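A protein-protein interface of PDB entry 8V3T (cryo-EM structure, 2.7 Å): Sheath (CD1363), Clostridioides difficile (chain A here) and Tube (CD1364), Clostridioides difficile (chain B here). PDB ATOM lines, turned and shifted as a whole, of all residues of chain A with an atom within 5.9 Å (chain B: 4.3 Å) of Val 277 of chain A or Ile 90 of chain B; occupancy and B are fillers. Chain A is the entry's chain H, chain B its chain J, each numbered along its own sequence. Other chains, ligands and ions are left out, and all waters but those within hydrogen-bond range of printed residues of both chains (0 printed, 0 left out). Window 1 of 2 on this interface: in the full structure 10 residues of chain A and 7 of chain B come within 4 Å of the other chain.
Hydrophobic or aromatic side chains of chain A within 4 Å of the printed part of chain B: Leu 274 and Val 277.
Of the 11 printed residues of chain B, 3 touch a printed residue of chain A.
Hydrophobic or aromatic side chains of chain B within 4 Å of the printed part of chain A: Ile 90 and Ala 105.
Among the printed residues, 5 pairs touch across the chains.
OG of Ser 281 of chain A lies within hydrogen-bond range of NZ of Lys 107 of chain B (3.1 Å).
Among the printed residues, merely in contact across the chains: Leu 274 of chain A with Ile 90 of chain B (3.7 Å), Lys 280 of chain A with Lys 107 of chain B (3.9 Å), Val 277 of chain A with Ile 90 of chain B (3.9 Å) and Val 277 of chain A with Ala 105 of chain B (3.96 Å).
Of the printed residues of chain B, Leu 274 of chain A touches Ile 90.
Of the printed residues of chain B, Lys 280 of chain A touches Lys 107.
Of the printed residues of chain B, Ser 281 of chain A touches Lys 107 (3.1 Å).
Of chain A, only Leu 274 (3.7 Å) and Val 277 (3.9 Å) come within 4 Å of Ile 90 of chain B.
Of the printed residues of chain A, Ala 105 of chain B touches Val 277.
The nearest residue of chain B that does not touch Val 277 of chain A is Val 88 of chain B (4.1 Å).
O of Val 277 of chain A lies within hydrogen-bond range of OG of Ser 281 of chain A.
The backbone NH (N) of Trp 18 of chain B sits at hydrogen-bond distance from the backbone carbonyl oxygen (O) of Ile 90 of chain B.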
ATOM      1  N   LYS A 272      -4.886  19.644   4.845  1.00  0.00           N
ATOM      2  CA  LYS A 272      -4.612  19.477   6.268  1.00  0.00           C
ATOM      3  C   LYS A 272      -5.812  19.895   7.107  1.00  0.00           C
ATOM      4  O   LYS A 272      -6.166  19.220   8.081  1.00  0.00           O
ATOM      5  CB  LYS A 272      -3.378  20.287   6.660  1.00  0.00           C
ATOM      6  CG  LYS A 272      -2.074  19.749   6.104  1.00  0.00           C
ATOM      7  CD  LYS A 272      -0.915  20.655   6.473  1.00  0.00           C
ATOM      8  CE  LYS A 272       0.399  20.117   5.941  1.00  0.00           C
ATOM      9  NZ  LYS A 272       1.565  20.858   6.491  1.00  0.00           N
ATOM     10  N   CYS A 273      -6.456  21.007   6.740  1.00  0.00           N
ATOM     11  CA  CYS A 273      -7.656  21.432   7.453  1.00  0.00           C
ATOM     12  C   CYS A 273      -8.776  20.409   7.309  1.00  0.00           C
ATOM     13  O   CYS A 273      -9.499  20.127   8.274  1.00  0.00           O
ATOM     14  CB  CYS A 273      -8.109  22.800   6.944  1.00  0.00           C
ATOM     15  SG  CYS A 273      -6.959  24.139   7.308  1.00  0.00           S
ATOM     16  N   LEU A 274      -8.939  19.847   6.108  1.00  0.00           N
ATOM     17  CA  LEU A 274      -9.958  18.817   5.910  1.00  0.00           C
ATOM     18  C   LEU A 274      -9.704  17.608   6.807  1.00  0.00           C
ATOM     19  O   LEU A 274     -10.630  17.083   7.445  1.00  0.00           O
ATOM     20  CB  LEU A 274      -9.990  18.394   4.441  1.00  0.00           C
ATOM     21  CG  LEU A 274     -10.548  19.389   3.421  1.00  0.00           C
ATOM     22  CD1 LEU A 274     -10.077  19.034   2.021  1.00  0.00           C
ATOM     23  CD2 LEU A 274     -12.065  19.428   3.474  1.00  0.00           C
ATOM     24  N   LEU A 275      -8.446  17.163   6.875  1.00  0.00           N
ATOM     25  CA  LEU A 275      -8.097  16.026   7.722  1.00  0.00           C
ATOM     26  C   LEU A 275      -8.343  16.335   9.195  1.00  0.00           C
ATOM     27  O   LEU A 275      -8.844  15.484   9.944  1.00  0.00           O
ATOM     28  CB  LEU A 275      -6.637  15.641   7.482  1.00  0.00           C
ATOM     29  CG  LEU A 275      -6.063  14.417   8.193  1.00  0.00           C
ATOM     30  CD1 LEU A 275      -6.774  13.150   7.757  1.00  0.00           C
ATOM     31  CD2 LEU A 275      -4.574  14.318   7.920  1.00  0.00           C
ATOM     32  N   ILE A 276      -8.000  17.551   9.626  1.00  0.00           N
ATOM     33  CA  ILE A 276      -8.235  17.948  11.013  1.00  0.00           C
ATOM     34  C   ILE A 276      -9.723  17.907  11.333  1.00  0.00           C
ATOM     35  O   ILE A 276     -10.131  17.428  12.399  1.00  0.00           O
ATOM     36  CB  ILE A 276      -7.638  19.342  11.278  1.00  0.00           C
ATOM     37  CG1 ILE A 276      -6.112  19.276  11.317  1.00  0.00           C
ATOM     38  CG2 ILE A 276      -8.169  19.918  12.579  1.00  0.00           C
ATOM     39  CD1 ILE A 276      -5.450  20.630  11.255  1.00  0.00           C
ATOM     40  N   VAL A 277     -10.556  18.411  10.419  1.00  0.00           N
ATOM     41  CA  VAL A 277     -11.998  18.420  10.651  1.00  0.00           C
ATOM     42  C   VAL A 277     -12.532  16.998  10.772  1.00  0.00           C
ATOM     43  O   VAL A 277     -13.351  16.693  11.654  1.00  0.00           O
ATOM     44  CB  VAL A 277     -12.711  19.204   9.533  1.00  0.00           C
ATOM     45  CG1 VAL A 277     -14.176  18.813   9.453  1.00  0.00           C
ATOM     46  CG2 VAL A 277     -12.571  20.696   9.762  1.00  0.00           C
ATOM     47  N   ALA A 278     -12.081  16.102   9.888  1.00  0.00           N
ATOM     48  CA  ALA A 278     -12.534  14.715   9.960  1.00  0.00           C
ATOM     49  C   ALA A 278     -12.145  14.071  11.289  1.00  0.00           C
ATOM     50  O   ALA A 278     -12.964  13.390  11.927  1.00  0.00           O
ATOM     51  CB  ALA A 278     -11.968  13.918   8.786  1.00  0.00           C
ATOM     52  N   ILE A 279     -10.905  14.294  11.733  1.00  0.00           N
ATOM     53  CA  ILE A 279     -10.459  13.715  12.999  1.00  0.00           C
ATOM     54  C   ILE A 279     -11.274  14.274  14.161  1.00  0.00           C
ATOM     55  O   ILE A 279     -11.638  13.545  15.094  1.00  0.00           O
ATOM     56  CB  ILE A 279      -8.949  13.954  13.188  1.00  0.00           C
ATOM     57  CG1 ILE A 279      -8.147  13.040  12.260  1.00  0.00           C
ATOM     58  CG2 ILE A 279      -8.540  13.720  14.631  1.00  0.00           C
ATOM     59  CD1 ILE A 279      -6.675  13.365  12.199  1.00  0.00           C
ATOM     60  N   LYS A 280     -11.573  15.575  14.126  1.00  0.00           N
ATOM     61  CA  LYS A 280     -12.352  16.182  15.199  1.00  0.00           C
ATOM     62  C   LYS A 280     -13.758  15.596  15.269  1.00  0.00           C
ATOM     63  O   LYS A 280     -14.281  15.348  16.362  1.00  0.00           O
ATOM     64  CB  LYS A 280     -12.409  17.697  15.016  1.00  0.00           C
ATOM     65  CG  LYS A 280     -13.287  18.401  16.032  1.00  0.00           C
ATOM     66  CD  LYS A 280     -12.671  18.342  17.418  1.00  0.00           C
ATOM     67  CE  LYS A 280     -13.506  19.107  18.428  1.00  0.00           C
ATOM     68  NZ  LYS A 280     -13.424  20.576  18.213  1.00  0.00           N
ATOM     69  N   SER A 281     -14.392  15.378  14.114  1.00  0.00           N
ATOM     70  CA  SER A 281     -15.712  14.751  14.120  1.00  0.00           C
ATOM     71  C   SER A 281     -15.646  13.334  14.683  1.00  0.00           C
ATOM     72  O   SER A 281     -16.526  12.916  15.457  1.00  0.00           O
ATOM     73  CB  SER A 281     -16.298  14.744  12.710  1.00  0.00           C
ATOM     74  OG  SER A 281     -16.371  16.057  12.187  1.00  0.00           O
ATOM     75  N   TYR A 282     -14.604  12.583  14.314  1.00  0.00           N
ATOM     76  CA  TYR A 282     -14.452  11.239  14.861  1.00  0.00           C
ATOM     77  C   TYR A 282     -14.319  11.275  16.379  1.00  0.00           C
ATOM     78  O   TYR A 282     -14.901  10.439  17.080  1.00  0.00           O
ATOM     79  CB  TYR A 282     -13.247  10.537  14.237  1.00  0.00           C
ATOM     80  CG  TYR A 282     -13.007   9.160  14.811  1.00  0.00           C
ATOM     81  CD1 TYR A 282     -13.739   8.067  14.369  1.00  0.00           C
ATOM     82  CD2 TYR A 282     -12.060   8.954  15.803  1.00  0.00           C
ATOM     83  CE1 TYR A 282     -13.529   6.809  14.892  1.00  0.00           C
ATOM     84  CE2 TYR A 282     -11.845   7.700  16.335  1.00  0.00           C
ATOM     85  CZ  TYR A 282     -12.582   6.631  15.875  1.00  0.00           C
ATOM     86  OH  TYR A 282     -12.371   5.380  16.400  1.00  0.00           O
ATOM     87  N   GLU B  16     -13.958  30.828  -1.002  1.00  0.00           N
ATOM     88  CA  GLU B  16     -13.847  29.443  -1.429  1.00  0.00           C
ATOM     89  C   GLU B  16     -14.701  28.566  -0.528  1.00  0.00           C
ATOM     90  O   GLU B  16     -14.870  28.850   0.660  1.00  0.00           O
ATOM     91  CB  GLU B  16     -12.389  28.965  -1.409  1.00  0.00           C
ATOM     92  CG  GLU B  16     -11.447  29.836  -2.220  1.00  0.00           C
ATOM     93  CD  GLU B  16     -10.029  29.309  -2.239  1.00  0.00           C
ATOM     94  OE1 GLU B  16      -9.849  28.080  -2.339  1.00  0.00           O
ATOM     95  OE2 GLU B  16      -9.089  30.127  -2.158  1.00  0.00           O
ATOM     96  N   LEU B  17     -15.240  27.493  -1.102  1.00  0.00           N
ATOM     97  CA  LEU B  17     -16.136  26.599  -0.385  1.00  0.00           C
ATOM     98  C   LEU B  17     -15.767  25.149  -0.659  1.00  0.00           C
ATOM     99  O   LEU B  17     -15.449  24.782  -1.792  1.00  0.00           O
ATOM    100  CB  LEU B  17     -17.597  26.850  -0.779  1.00  0.00           C
ATOM    101  CG  LEU B  17     -18.671  26.177   0.078  1.00  0.00           C
ATOM    102  CD1 LEU B  17     -18.718  26.793   1.463  1.00  0.00           C
ATOM    103  CD2 LEU B  17     -20.028  26.270  -0.594  1.00  0.00           C
ATOM    104  N   TRP B  18     -15.802  24.334   0.392  1.00  0.00           N
ATOM    105  CA  TRP B  18     -15.678  22.887   0.292  1.00  0.00           C
ATOM    106  C   TRP B  18     -16.958  22.267   0.828  1.00  0.00           C
ATOM    107  O   TRP B  18     -17.351  22.543   1.965  1.00  0.00           O
ATOM    108  CB  TRP B  18     -14.474  22.369   1.087  1.00  0.00           C
ATOM    109  CG  TRP B  18     -13.147  22.557   0.416  1.00  0.00           C
ATOM    110  CD1 TRP B  18     -12.496  21.659  -0.375  1.00  0.00           C
ATOM    111  CD2 TRP B  18     -12.296  23.705   0.502  1.00  0.00           C
ATOM    112  NE1 TRP B  18     -11.301  22.180  -0.799  1.00  0.00           N
ATOM    113  CE2 TRP B  18     -11.153  23.436  -0.274  1.00  0.00           C
ATOM    114  CE3 TRP B  18     -12.393  24.938   1.153  1.00  0.00           C
ATOM    115  CZ2 TRP B  18     -10.116  24.353  -0.417  1.00  0.00           C
ATOM    116  CZ3 TRP B  18     -11.364  25.846   1.010  1.00  0.00           C
ATOM    117  CH2 TRP B  18     -10.240  25.549   0.232  1.00  0.00           C
ATOM    118  N   VAL B  88     -20.843  18.235   5.690  1.00  0.00           N
ATOM    119  CA  VAL B  88     -19.912  19.158   6.328  1.00  0.00           C
ATOM    120  C   VAL B  88     -19.428  20.150   5.280  1.00  0.00           C
ATOM    121  O   VAL B  88     -19.116  19.764   4.148  1.00  0.00           O
ATOM    122  CB  VAL B  88     -18.722  18.411   6.967  1.00  0.00           C
ATOM    123  CG1 VAL B  88     -17.676  19.390   7.466  1.00  0.00           C
ATOM    124  CG2 VAL B  88     -19.198  17.515   8.097  1.00  0.00           C
ATOM    125  N   ALA B  89     -19.367  21.428   5.652  1.00  0.00           N
ATOM    126  CA  ALA B  89     -18.917  22.481   4.751  1.00  0.00           C
ATOM    127  C   ALA B  89     -17.816  23.299   5.410  1.00  0.00           C
ATOM    128  O   ALA B  89     -17.854  23.549   6.617  1.00  0.00           O
ATOM    129  CB  ALA B  89     -20.069  23.402   4.344  1.00  0.00           C
ATOM    130  N   ILE B  90     -16.838  23.712   4.609  1.00  0.00           N
ATOM    131  CA  ILE B  90     -15.737  24.553   5.065  1.00  0.00           C
ATOM    132  C   ILE B  90     -15.655  25.762   4.146  1.00  0.00           C
ATOM    133  O   ILE B  90     -15.520  25.608   2.926  1.00  0.00           O
ATOM    134  CB  ILE B  90     -14.398  23.799   5.081  1.00  0.00           C
ATOM    135  CG1 ILE B  90     -14.421  22.689   6.133  1.00  0.00           C
ATOM    136  CG2 ILE B  90     -13.249  24.760   5.338  1.00  0.00           C
ATOM    137  CD1 ILE B  90     -13.252  21.742   6.046  1.00  0.00           C
ATOM    138  N   SER B  91     -15.731  26.956   4.722  1.00  0.00           N
ATOM    139  CA  SER B  91     -15.647  28.200   3.975  1.00  0.00           C
ATOM    140  C   SER B  91     -14.357  28.927   4.325  1.00  0.00           C
ATOM    141  O   SER B  91     -13.918  28.913   5.478  1.00  0.00           O
ATOM    142  CB  SER B  91     -16.850  29.101   4.264  1.00  0.00           C
ATOM    143  OG  SER B  91     -16.602  29.941   5.374  1.00  0.00           O
ATOM    144  N   ILE B 104     -13.924  28.526   8.566  1.00  0.00           N
ATOM    145  CA  ILE B 104     -14.945  28.020   9.475  1.00  0.00           C
ATOM    146  C   ILE B 104     -15.511  26.730   8.905  1.00  0.00           C
ATOM    147  O   ILE B 104     -15.758  26.625   7.700  1.00  0.00           O
ATOM    148  CB  ILE B 104     -16.064  29.055   9.725  1.00  0.00           C
ATOM    149  CG1 ILE B 104     -15.476  30.359  10.268  1.00  0.00           C
ATOM    150  CG2 ILE B 104     -17.096  28.510  10.695  1.00  0.00           C
ATOM    151  CD1 ILE B 104     -16.489  31.420  10.540  1.00  0.00           C
ATOM    152  N   ALA B 105     -15.705  25.744   9.774  1.00  0.00           N
ATOM    153  CA  ALA B 105     -16.338  24.486   9.414  1.00  0.00           C
ATOM    154  C   ALA B 105     -17.761  24.481   9.951  1.00  0.00           C
ATOM    155  O   ALA B 105     -17.985  24.785  11.126  1.00  0.00           O
ATOM    156  CB  ALA B 105     -15.555  23.296   9.969  1.00  0.00           C
ATOM    157  N   LYS B 107     -21.121  22.039  10.357  1.00  0.00           N
ATOM    158  CA  LYS B 107     -21.301  20.601  10.464  1.00  0.00           C
ATOM    159  C   LYS B 107     -22.761  20.253  10.710  1.00  0.00           C
ATOM    160  O   LYS B 107     -23.558  21.089  11.144  1.00  0.00           O
ATOM    161  CB  LYS B 107     -20.437  20.018  11.588  1.00  0.00           C
ATOM    162  CG  LYS B 107     -18.959  20.320  11.456  1.00  0.00           C
ATOM    163  CD  LYS B 107     -18.246  20.115  12.777  1.00  0.00           C
ATOM    164  CE  LYS B 107     -16.953  19.348  12.588  1.00  0.00           C
ATOM    165  NZ  LYS B 107     -16.512  18.703  13.855  1.00  0.00           N
ATOM    166  N   LEU B 139     -11.287  27.746  12.630  1.00  0.00           N
ATOM    167  CA  LEU B 139      -9.939  27.550  12.116  1.00  0.00           C
ATOM    168  C   LEU B 139      -9.418  28.882  11.595  1.00  0.00           C
ATOM    169  O   LEU B 139     -10.088  29.540  10.796  1.00  0.00           O
ATOM    170  CB  LEU B 139      -9.918  26.501  10.999  1.00  0.00           C
ATOM    171  CG  LEU B 139     -10.705  25.206  11.213  1.00  0.00           C
ATOM    172  CD1 LEU B 139     -11.149  24.623   9.880  1.00  0.00           C
ATOM    173  CD2 LEU B 139      -9.888  24.189  11.991  1.00  0.00           C
